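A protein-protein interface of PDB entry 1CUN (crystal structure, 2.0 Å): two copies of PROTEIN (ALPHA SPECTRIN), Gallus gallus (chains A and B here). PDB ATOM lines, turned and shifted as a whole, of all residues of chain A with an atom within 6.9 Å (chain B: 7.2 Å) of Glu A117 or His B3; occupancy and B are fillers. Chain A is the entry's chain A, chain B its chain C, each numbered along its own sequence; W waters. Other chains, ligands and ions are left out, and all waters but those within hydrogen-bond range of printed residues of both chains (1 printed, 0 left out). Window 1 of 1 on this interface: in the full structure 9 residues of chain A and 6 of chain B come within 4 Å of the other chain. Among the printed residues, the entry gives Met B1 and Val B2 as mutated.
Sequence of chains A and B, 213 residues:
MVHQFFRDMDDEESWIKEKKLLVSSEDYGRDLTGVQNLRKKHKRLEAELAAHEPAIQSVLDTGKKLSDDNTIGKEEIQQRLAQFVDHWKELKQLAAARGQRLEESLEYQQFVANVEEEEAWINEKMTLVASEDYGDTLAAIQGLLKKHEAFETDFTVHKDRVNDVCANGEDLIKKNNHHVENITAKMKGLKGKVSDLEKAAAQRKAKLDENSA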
ATOM      1  N   LEU A  32      31.428  22.289  24.945  1.00  0.00           N
ATOM      2  CA  LEU A  32      30.651  21.600  23.926  1.00  0.00           C
ATOM      3  C   LEU A  32      31.464  21.197  22.681  1.00  0.00           C
ATOM      4  O   LEU A  32      31.434  20.035  22.282  1.00  0.00           O
ATOM      5  CB  LEU A  32      29.463  22.464  23.479  1.00  0.00           C
ATOM      6  CG  LEU A  32      28.136  21.753  23.197  1.00  0.00           C
ATOM      7  CD1 LEU A  32      27.239  22.618  22.325  1.00  0.00           C
ATOM      8  CD2 LEU A  32      28.367  20.400  22.558  1.00  0.00           C
ATOM      9  N   GLN A 110      26.134  20.543  26.792  1.00  0.00           N
ATOM     10  CA  GLN A 110      25.021  21.200  26.100  1.00  0.00           C
ATOM     11  C   GLN A 110      24.264  22.066  27.138  1.00  0.00           C
ATOM     12  O   GLN A 110      23.929  23.225  26.868  1.00  0.00           O
ATOM     13  CB  GLN A 110      24.064  20.168  25.453  1.00  0.00           C
ATOM     14  CG  GLN A 110      24.566  19.614  24.108  1.00  0.00           C
ATOM     15  CD  GLN A 110      23.543  18.760  23.341  1.00  0.00           C
ATOM     16  OE1 GLN A 110      22.332  18.827  23.584  1.00  0.00           O
ATOM     17  NE2 GLN A 110      24.033  17.975  22.388  1.00  0.00           N
ATOM     18  N   PHE A 111      24.013  21.510  28.321  1.00  0.00           N
ATOM     19  CA  PHE A 111      23.342  22.241  29.405  1.00  0.00           C
ATOM     20  C   PHE A 111      24.189  23.487  29.785  1.00  0.00           C
ATOM     21  O   PHE A 111      23.665  24.601  29.904  1.00  0.00           O
ATOM     22  CB  PHE A 111      23.177  21.317  30.625  1.00  0.00           C
ATOM     23  CG  PHE A 111      22.820  22.041  31.901  1.00  0.00           C
ATOM     24  CD1 PHE A 111      21.494  22.348  32.205  1.00  0.00           C
ATOM     25  CD2 PHE A 111      23.817  22.429  32.789  1.00  0.00           C
ATOM     26  CE1 PHE A 111      21.168  23.038  33.385  1.00  0.00           C
ATOM     27  CE2 PHE A 111      23.498  23.113  33.957  1.00  0.00           C
ATOM     28  CZ  PHE A 111      22.165  23.418  34.254  1.00  0.00           C
ATOM     29  N   VAL A 112      25.498  23.305  29.970  1.00  0.00           N
ATOM     30  CA  VAL A 112      26.352  24.452  30.299  1.00  0.00           C
ATOM     31  C   VAL A 112      26.253  25.505  29.179  1.00  0.00           C
ATOM     32  O   VAL A 112      26.131  26.706  29.451  1.00  0.00           O
ATOM     33  CB  VAL A 112      27.844  24.033  30.502  1.00  0.00           C
ATOM     34  CG1 VAL A 112      28.744  25.279  30.727  1.00  0.00           C
ATOM     35  CG2 VAL A 112      27.947  23.068  31.697  1.00  0.00           C
ATOM     36  N   ALA A 113      26.264  25.064  27.923  1.00  0.00           N
ATOM     37  CA  ALA A 113      26.175  26.011  26.808  1.00  0.00           C
ATOM     38  C   ALA A 113      24.800  26.699  26.769  1.00  0.00           C
ATOM     39  O   ALA A 113      24.695  27.905  26.492  1.00  0.00           O
ATOM     40  CB  ALA A 113      26.440  25.292  25.460  1.00  0.00           C
ATOM     41  N   ASN A 114      23.751  25.932  27.048  1.00  0.00           N
ATOM     42  CA  ASN A 114      22.396  26.487  27.010  1.00  0.00           C
ATOM     43  C   ASN A 114      22.205  27.530  28.107  1.00  0.00           C
ATOM     44  O   ASN A 114      21.525  28.532  27.905  1.00  0.00           O
ATOM     45  CB  ASN A 114      21.343  25.375  27.180  1.00  0.00           C
ATOM     46  CG  ASN A 114      21.342  24.373  26.041  1.00  0.00           C
ATOM     47  OD1 ASN A 114      20.740  23.283  26.149  1.00  0.00           O
ATOM     48  ND2 ASN A 114      21.993  24.724  24.946  1.00  0.00           N
ATOM     49  N   VAL A 115      22.784  27.283  29.276  1.00  0.00           N
ATOM     50  CA  VAL A 115      22.680  28.226  30.385  1.00  0.00           C
ATOM     51  C   VAL A 115      23.365  29.535  30.011  1.00  0.00           C
ATOM     52  O   VAL A 115      22.865  30.622  30.315  1.00  0.00           O
ATOM     53  CB  VAL A 115      23.332  27.673  31.645  1.00  0.00           C
ATOM     54  CG1 VAL A 115      23.512  28.781  32.702  1.00  0.00           C
ATOM     55  CG2 VAL A 115      22.483  26.550  32.196  1.00  0.00           C
ATOM     56  N   GLU A 116      24.514  29.441  29.359  1.00  0.00           N
ATOM     57  CA  GLU A 116      25.213  30.660  28.963  1.00  0.00           C
ATOM     58  C   GLU A 116      24.415  31.441  27.916  1.00  0.00           C
ATOM     59  O   GLU A 116      24.333  32.661  27.983  1.00  0.00           O
ATOM     60  CB  GLU A 116      26.626  30.338  28.435  1.00  0.00           C
ATOM     61  CG  GLU A 116      27.344  31.555  27.835  1.00  0.00           C
ATOM     62  CD  GLU A 116      27.596  32.682  28.850  1.00  0.00           C
ATOM     63  OE1 GLU A 116      28.000  33.790  28.421  1.00  0.00           O
ATOM     64  OE2 GLU A 116      27.403  32.474  30.068  1.00  0.00           O
ATOM     65  N   GLU A 117      23.819  30.751  26.951  1.00  0.00           N
ATOM     66  CA  GLU A 117      23.022  31.440  25.934  1.00  0.00           C
ATOM     67  C   GLU A 117      21.846  32.211  26.577  1.00  0.00           C
ATOM     68  O   GLU A 117      21.560  33.355  26.207  1.00  0.00           O
ATOM     69  CB  GLU A 117      22.484  30.435  24.885  1.00  0.00           C
ATOM     70  CG  GLU A 117      23.574  29.934  23.903  1.00  0.00           C
ATOM     71  CD  GLU A 117      23.058  28.938  22.854  1.00  0.00           C
ATOM     72  OE1 GLU A 117      21.818  28.772  22.735  1.00  0.00           O
ATOM     73  OE2 GLU A 117      23.897  28.327  22.145  1.00  0.00           O
ATOM     74  N   GLU A 118      21.170  31.591  27.542  1.00  0.00           N
ATOM     75  CA  GLU A 118      20.036  32.267  28.175  1.00  0.00           C
ATOM     76  C   GLU A 118      20.523  33.403  29.079  1.00  0.00           C
ATOM     77  O   GLU A 118      19.958  34.486  29.073  1.00  0.00           O
ATOM     78  CB  GLU A 118      19.179  31.263  28.965  1.00  0.00           C
ATOM     79  CG  GLU A 118      18.440  30.250  28.078  1.00  0.00           C
ATOM     80  CD  GLU A 118      17.581  30.893  26.982  1.00  0.00           C
ATOM     81  OE1 GLU A 118      17.041  32.006  27.180  1.00  0.00           O
ATOM     82  OE2 GLU A 118      17.421  30.271  25.908  1.00  0.00           O
ATOM     83  N   GLU A 119      21.575  33.170  29.848  1.00  0.00           N
ATOM     84  CA  GLU A 119      22.087  34.236  30.705  1.00  0.00           C
ATOM     85  C   GLU A 119      22.623  35.442  29.934  1.00  0.00           C
ATOM     86  O   GLU A 119      22.459  36.582  30.386  1.00  0.00           O
ATOM     87  CB  GLU A 119      23.144  33.694  31.661  1.00  0.00           C
ATOM     88  CG  GLU A 119      22.486  32.760  32.665  1.00  0.00           C
ATOM     89  CD  GLU A 119      23.268  32.569  33.939  1.00  0.00           C
ATOM     90  OE1 GLU A 119      22.611  32.253  34.965  1.00  0.00           O
ATOM     91  OE2 GLU A 119      24.522  32.709  33.918  1.00  0.00           O
ATOM     92  N   ALA A 120      23.254  35.212  28.781  1.00  0.00           N
ATOM     93  CA  ALA A 120      23.772  36.341  28.001  1.00  0.00           C
ATOM     94  C   ALA A 120      22.584  37.165  27.501  1.00  0.00           C
ATOM     95  O   ALA A 120      22.631  38.396  27.510  1.00  0.00           O
ATOM     96  CB  ALA A 120      24.627  35.863  26.807  1.00  0.00           C
ATOM     97  N   TRP A 121      21.525  36.492  27.062  1.00  0.00           N
ATOM     98  CA  TRP A 121      20.346  37.205  26.574  1.00  0.00           C
ATOM     99  C   TRP A 121      19.749  38.039  27.722  1.00  0.00           C
ATOM    100  O   TRP A 121      19.452  39.224  27.564  1.00  0.00           O
ATOM    101  CB  TRP A 121      19.301  36.216  26.040  1.00  0.00           C
ATOM    102  CG  TRP A 121      18.127  36.884  25.382  1.00  0.00           C
ATOM    103  CD1 TRP A 121      18.040  37.303  24.081  1.00  0.00           C
ATOM    104  CD2 TRP A 121      16.900  37.274  26.014  1.00  0.00           C
ATOM    105  NE1 TRP A 121      16.830  37.930  23.869  1.00  0.00           N
ATOM    106  CE2 TRP A 121      16.116  37.927  25.040  1.00  0.00           C
ATOM    107  CE3 TRP A 121      16.386  37.132  27.313  1.00  0.00           C
ATOM    108  CZ2 TRP A 121      14.840  38.444  25.322  1.00  0.00           C
ATOM    109  CZ3 TRP A 121      15.114  37.646  27.594  1.00  0.00           C
ATOM    110  CH2 TRP A 121      14.363  38.293  26.597  1.00  0.00           C
ATOM    111  N   ILE A 122      19.618  37.424  28.890  1.00  0.00           N
ATOM    112  CA  ILE A 122      19.057  38.101  30.045  1.00  0.00           C
ATOM    113  C   ILE A 122      19.929  39.291  30.451  1.00  0.00           C
ATOM    114  O   ILE A 122      19.422  40.394  30.712  1.00  0.00           O
ATOM    115  CB  ILE A 122      18.876  37.104  31.237  1.00  0.00           C
ATOM    116  CG1 ILE A 122      17.792  36.064  30.871  1.00  0.00           C
ATOM    117  CG2 ILE A 122      18.491  37.851  32.514  1.00  0.00           C
ATOM    118  CD1 ILE A 122      17.610  34.937  31.926  1.00  0.00           C
ATOM    119  N   HIS A 158      11.733  33.121  25.959  1.00  0.00           N
ATOM    120  CA  HIS A 158      12.919  32.758  26.729  1.00  0.00           C
ATOM    121  C   HIS A 158      12.587  32.152  28.091  1.00  0.00           C
ATOM    122  O   HIS A 158      13.351  31.328  28.598  1.00  0.00           O
ATOM    123  CB  HIS A 158      13.857  33.968  26.894  1.00  0.00           C
ATOM    124  CG  HIS A 158      14.620  34.304  25.646  1.00  0.00           C
ATOM    125  ND1 HIS A 158      15.797  33.671  25.301  1.00  0.00           N
ATOM    126  CD2 HIS A 158      14.336  35.153  24.626  1.00  0.00           C
ATOM    127  CE1 HIS A 158      16.203  34.114  24.122  1.00  0.00           C
ATOM    128  NE2 HIS A 158      15.334  35.012  23.690  1.00  0.00           N
ATOM    129  N   ARG A 161      12.145  28.592  27.393  1.00  0.00           N
ATOM    130  CA  ARG A 161      13.438  27.940  27.129  1.00  0.00           C
ATOM    131  C   ARG A 161      14.187  27.719  28.455  1.00  0.00           C
ATOM    132  O   ARG A 161      14.840  26.689  28.650  1.00  0.00           O
ATOM    133  CB  ARG A 161      14.278  28.779  26.157  1.00  0.00           C
ATOM    134  CG  ARG A 161      13.753  28.715  24.713  1.00  0.00           C
ATOM    135  CD  ARG A 161      14.550  29.595  23.765  1.00  0.00           C
ATOM    136  NE  ARG A 161      13.884  29.740  22.470  1.00  0.00           N
ATOM    137  CZ  ARG A 161      14.271  30.575  21.509  1.00  0.00           C
ATOM    138  NH1 ARG A 161      15.338  31.348  21.676  1.00  0.00           N
ATOM    139  NH2 ARG A 161      13.559  30.676  20.397  1.00  0.00           N
ATOM    140  N   VAL A 162      14.087  28.673  29.377  1.00  0.00           N
ATOM    141  CA  VAL A 162      14.758  28.492  30.653  1.00  0.00           C
ATOM    142  C   VAL A 162      14.131  27.299  31.387  1.00  0.00           C
ATOM    143  O   VAL A 162      14.848  26.489  31.981  1.00  0.00           O
ATOM    144  CB  VAL A 162      14.692  29.771  31.541  1.00  0.00           C
ATOM    145  CG1 VAL A 162      15.068  29.430  32.964  1.00  0.00           C
ATOM    146  CG2 VAL A 162      15.665  30.840  31.010  1.00  0.00           C
ATOM    147  N   ASP A 164      12.891  24.655  30.133  1.00  0.00           N
ATOM    148  CA  ASP A 164      13.431  23.463  29.486  1.00  0.00           C
ATOM    149  C   ASP A 164      14.868  23.186  29.902  1.00  0.00           C
ATOM    150  O   ASP A 164      15.204  22.046  30.179  1.00  0.00           O
ATOM    151  CB  ASP A 164      13.339  23.575  27.966  1.00  0.00           C
ATOM    152  CG  ASP A 164      11.931  23.331  27.463  1.00  0.00           C
ATOM    153  OD1 ASP A 164      11.056  22.976  28.290  1.00  0.00           O
ATOM    154  OD2 ASP A 164      11.703  23.485  26.246  1.00  0.00           O
ATOM    155  N   VAL A 165      15.710  24.221  29.947  1.00  0.00           N
ATOM    156  CA  VAL A 165      17.094  24.038  30.388  1.00  0.00           C
ATOM    157  C   VAL A 165      17.120  23.489  31.817  1.00  0.00           C
ATOM    158  O   VAL A 165      17.946  22.631  32.152  1.00  0.00           O
ATOM    159  CB  VAL A 165      17.884  25.374  30.355  1.00  0.00           C
ATOM    160  CG1 VAL A 165      19.240  25.194  30.990  1.00  0.00           C
ATOM    161  CG2 VAL A 165      18.043  25.841  28.927  1.00  0.00           C
ATOM    162  N   LEU A 190      20.046  30.778  37.131  1.00  0.00           N
ATOM    163  CA  LEU A 190      19.268  31.119  35.958  1.00  0.00           C
ATOM    164  C   LEU A 190      17.832  31.550  36.330  1.00  0.00           C
ATOM    165  O   LEU A 190      17.333  32.552  35.824  1.00  0.00           O
ATOM    166  CB  LEU A 190      19.272  29.926  34.990  1.00  0.00           C
ATOM    167  CG  LEU A 190      18.707  30.065  33.583  1.00  0.00           C
ATOM    168  CD1 LEU A 190      19.353  31.248  32.837  1.00  0.00           C
ATOM    169  CD2 LEU A 190      18.935  28.748  32.840  1.00  0.00           C
ATOM    170  N   MET B   1      16.277  20.570  23.680  1.00  0.00           N
ATOM    171  CA  MET B   1      16.350  20.163  22.247  1.00  0.00           C
ATOM    172  C   MET B   1      16.359  21.371  21.312  1.00  0.00           C
ATOM    173  O   MET B   1      17.042  21.355  20.282  1.00  0.00           O
ATOM    174  CB  MET B   1      15.164  19.255  21.897  1.00  0.00           C
ATOM    175  CG  MET B   1      15.197  18.709  20.473  1.00  0.00           C
ATOM    176  SD  MET B   1      13.823  17.567  20.134  1.00  0.00           S
ATOM    177  CE  MET B   1      14.377  16.106  21.106  1.00  0.00           C
ATOM    178  N   VAL B   2      15.618  22.420  21.680  1.00  0.00           N
ATOM    179  CA  VAL B   2      15.541  23.617  20.851  1.00  0.00           C
ATOM    180  C   VAL B   2      16.883  24.346  20.678  1.00  0.00           C
ATOM    181  O   VAL B   2      17.185  24.814  19.587  1.00  0.00           O
ATOM    182  CB  VAL B   2      14.485  24.608  21.396  1.00  0.00           C
ATOM    183  CG1 VAL B   2      14.901  25.125  22.770  1.00  0.00           C
ATOM    184  CG2 VAL B   2      14.294  25.744  20.412  1.00  0.00           C
ATOM    185  N   HIS B   3      17.677  24.437  21.747  1.00  0.00           N
ATOM    186  CA  HIS B   3      18.990  25.103  21.688  1.00  0.00           C
ATOM    187  C   HIS B   3      19.935  24.386  20.714  1.00  0.00           C
ATOM    188  O   HIS B   3      20.586  25.031  19.900  1.00  0.00           O
ATOM    189  CB  HIS B   3      19.662  25.113  23.064  1.00  0.00           C
ATOM    190  CG  HIS B   3      18.960  25.957  24.078  1.00  0.00           C
ATOM    191  ND1 HIS B   3      19.183  27.311  24.205  1.00  0.00           N
ATOM    192  CD2 HIS B   3      17.995  25.648  24.974  1.00  0.00           C
ATOM    193  CE1 HIS B   3      18.382  27.801  25.134  1.00  0.00           C
ATOM    194  NE2 HIS B   3      17.650  26.812  25.614  1.00  0.00           N
ATOM    195  N   GLN B   4      20.019  23.061  20.820  1.00  0.00           N
ATOM    196  CA  GLN B   4      20.900  22.296  19.944  1.00  0.00           C
ATOM    197  C   GLN B   4      20.383  22.338  18.506  1.00  0.00           C
ATOM    198  O   GLN B   4      21.165  22.380  17.557  1.00  0.00           O
ATOM    199  CB  GLN B   4      21.036  20.844  20.431  1.00  0.00           C
ATOM    200  CG  GLN B   4      22.122  20.048  19.670  1.00  0.00           C
ATOM    201  CD  GLN B   4      23.494  20.712  19.759  1.00  0.00           C
ATOM    202  OE1 GLN B   4      24.182  20.919  18.743  1.00  0.00           O
ATOM    203  NE2 GLN B   4      23.890  21.055  20.959  1.00  0.00           N
ATOM    204  N   PHE B   5      19.064  22.340  18.347  1.00  0.00           N
ATOM    205  CA  PHE B   5      18.462  22.424  17.022  1.00  0.00           C
ATOM    206  C   PHE B   5      18.916  23.727  16.337  1.00  0.00           C
ATOM    207  O   PHE B   5      19.325  23.714  15.176  1.00  0.00           O
ATOM    208  CB  PHE B   5      16.922  22.358  17.145  1.00  0.00           C
ATOM    209  CG  PHE B   5      16.175  22.852  15.936  1.00  0.00           C
ATOM    210  CD1 PHE B   5      16.051  22.061  14.793  1.00  0.00           C
ATOM    211  CD2 PHE B   5      15.569  24.112  15.949  1.00  0.00           C
ATOM    212  CE1 PHE B   5      15.331  22.516  13.673  1.00  0.00           C
ATOM    213  CE2 PHE B   5      14.843  24.581  14.836  1.00  0.00           C
ATOM    214  CZ  PHE B   5      14.723  23.780  13.698  1.00  0.00           C
ATOM    215  N   PHE B   6      18.878  24.853  17.045  1.00  0.00           N
ATOM    216  CA  PHE B   6      19.296  26.096  16.412  1.00  0.00           C
ATOM    217  C   PHE B   6      20.804  26.115  16.106  1.00  0.00           C
ATOM    218  O   PHE B   6      21.225  26.680  15.089  1.00  0.00           O
ATOM    219  CB  PHE B   6      18.864  27.308  17.250  1.00  0.00           C
ATOM    220  CG  PHE B   6      17.419  27.724  17.015  1.00  0.00           C
ATOM    221  CD1 PHE B   6      16.525  27.843  18.074  1.00  0.00           C
ATOM    222  CD2 PHE B   6      16.969  28.012  15.738  1.00  0.00           C
ATOM    223  CE1 PHE B   6      15.209  28.239  17.862  1.00  0.00           C
ATOM    224  CE2 PHE B   6      15.642  28.418  15.509  1.00  0.00           C
ATOM    225  CZ  PHE B   6      14.765  28.528  16.583  1.00  0.00           C
ATOM    226  N   ARG B   7      21.604  25.490  16.961  1.00  0.00           N
ATOM    227  CA  ARG B   7      23.033  25.423  16.720  1.00  0.00           C
ATOM    228  C   ARG B   7      23.308  24.556  15.482  1.00  0.00           C
ATOM    229  O   ARG B   7      24.113  24.921  14.626  1.00  0.00           O
ATOM    230  CB  ARG B   7      23.766  24.841  17.937  1.00  0.00           C
ATOM    231  CG  ARG B   7      23.941  25.830  19.107  1.00  0.00           C
ATOM    232  CD  ARG B   7      24.943  25.295  20.131  1.00  0.00           C
ATOM    233  NE  ARG B   7      24.430  24.166  20.908  1.00  0.00           N
ATOM    234  CZ  ARG B   7      23.700  24.277  22.018  1.00  0.00           C
ATOM    235  NH1 ARG B   7      23.285  23.184  22.652  1.00  0.00           N
ATOM    236  NH2 ARG B   7      23.403  25.479  22.506  1.00  0.00           N
ATOM    237  N   ASP B   8      22.652  23.408  15.390  1.00  0.00           N
ATOM    238  CA  ASP B   8      22.852  22.535  14.237  1.00  0.00           C
ATOM    239  C   ASP B   8      22.373  23.175  12.944  1.00  0.00           C
ATOM    240  O   ASP B   8      23.028  23.055  11.902  1.00  0.00           O
ATOM    241  CB  ASP B   8      22.146  21.188  14.446  1.00  0.00           C
ATOM    242  CG  ASP B   8      22.786  20.378  15.539  1.00  0.00           C
ATOM    243  OD1 ASP B   8      23.920  20.739  15.936  1.00  0.00           O
ATOM    244  OD2 ASP B   8      22.180  19.389  16.003  1.00  0.00           O
ATOM    245  N   MET B   9      21.240  23.867  13.005  1.00  0.00           N
ATOM    246  CA  MET B   9      20.724  24.517  11.813  1.00  0.00           C
ATOM    247  C   MET B   9      21.673  25.629  11.369  1.00  0.00           C
ATOM    248  O   MET B   9      21.932  25.796  10.177  1.00  0.00           O
ATOM    249  CB  MET B   9      19.325  25.074  12.058  1.00  0.00           C
ATOM    250  CG  MET B   9      18.692  25.707  10.826  1.00  0.00           C
ATOM    251  SD  MET B   9      16.898  26.034  11.031  1.00  0.00           S
ATOM    252  CE  MET B   9      16.956  27.295  12.228  1.00  0.00           C
ATOM    253  N   LEU B  66       9.645  19.574  16.970  1.00  0.00           N
ATOM    254  CA  LEU B  66       9.575  20.739  17.846  1.00  0.00           C
ATOM    255  C   LEU B  66       8.384  21.617  17.502  1.00  0.00           C
ATOM    256  O   LEU B  66       7.719  22.152  18.390  1.00  0.00           O
ATOM    257  CB  LEU B  66      10.853  21.575  17.744  1.00  0.00           C
ATOM    258  CG  LEU B  66      12.158  20.939  18.222  1.00  0.00           C
ATOM    259  CD1 LEU B  66      13.305  21.895  17.946  1.00  0.00           C
ATOM    260  CD2 LEU B  66      12.067  20.615  19.703  1.00  0.00           C
HETATM  261  O   HOH W   1      20.839  27.747  20.522  1.00  0.00           O
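Of chain B, only His B3 (3.4 Å) and Arg B7 (2.9 Å) come within 4 Å of Glu A117. Printed residues of chain B within 4 Å of Gln A110: Gln B4 (3.3 Å). Of the printed residues of chain A, Arg B7 touches Leu A32 (3.5 Å), Asn A114 (2.9 Å) and Glu A117 (2.9 Å). Of the printed residues of chain A, Phe B6 touches Arg A161 (3.9 Å). Val A162 touches none of the printed residues of chain B. Met B1 touches none of the printed residues of chain A. The nearest residue of chain B that does not touch Glu A117 is Gln B4 (6.3 Å). The nearest printed residue of chain B that does not touch Leu A32 is Asp B8 (7.4 Å).
Among the printed residues, merely in contact across the chains: Leu A32 with Gln B4, Leu A32 with Arg B7, Asn A114 with His B3, Arg A161 with His B3, Arg A161 with Phe B6 and Val A165 with His B3.
No position is printed for both chains. Of the 11 pairs that touch across the chains among the printed residues, none has its exchanged pair printed and touching as well.
Printed residues of chain B that touch a printed residue of chain A: His B3, Gln B4, Phe B6 and Arg B7. Hydrophobic or aromatic side chains of chain B that line the printed part of chain A: His B3 and Phe B6. Along chain B the printed residues that touch a printed residue of chain A span positions 3 to 7. Hydrophobic or aromatic side chains of chain A that line the printed part of chain B: Leu A32 and Val A165.
The backbone carbonyl oxygen (O) of Gln A110 lies close to the side-chain amide nitrogen (ND2) of Asn A114 (3.1 Å). A ring nitrogen (ND1) of His A158 lies within hydrogen-bond range of the side-chain carboxylate (OE1) of Glu A118 (2.8 Å). The side-chain amide nitrogen of Gln B4 sits close to the guanidinium group of Arg B7, 2.8 Å away. OD1 of Asp B8 sits close to OE1 of Gln B4 (2.8 Å).
Water W1 bridges the side-chain carboxylate (OE1) of Glu A117 (2.6 Å) and the backbone carbonyl oxygen (O) of His B3 (2.8 Å).
NE2 of Gln B4 lies close to NE2 of Gln A110 (3.4 Å). The guanidinium group (NH2) of Arg B7 lies close to the side-chain amide nitrogen (ND2) of Asn A114 (2.9 Å). The side-chain carboxylate (OE1) of Glu A117 sits at hydrogen-bond distance from a ring nitrogen (ND1) of His B3. OE2 of Glu A117 lies within salt-bridge range of NH2 of Arg B7 (2.9 Å). A ring nitrogen (NE2) of His B3 sits close to the side-chain carboxylate (OE2) of Glu A118.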
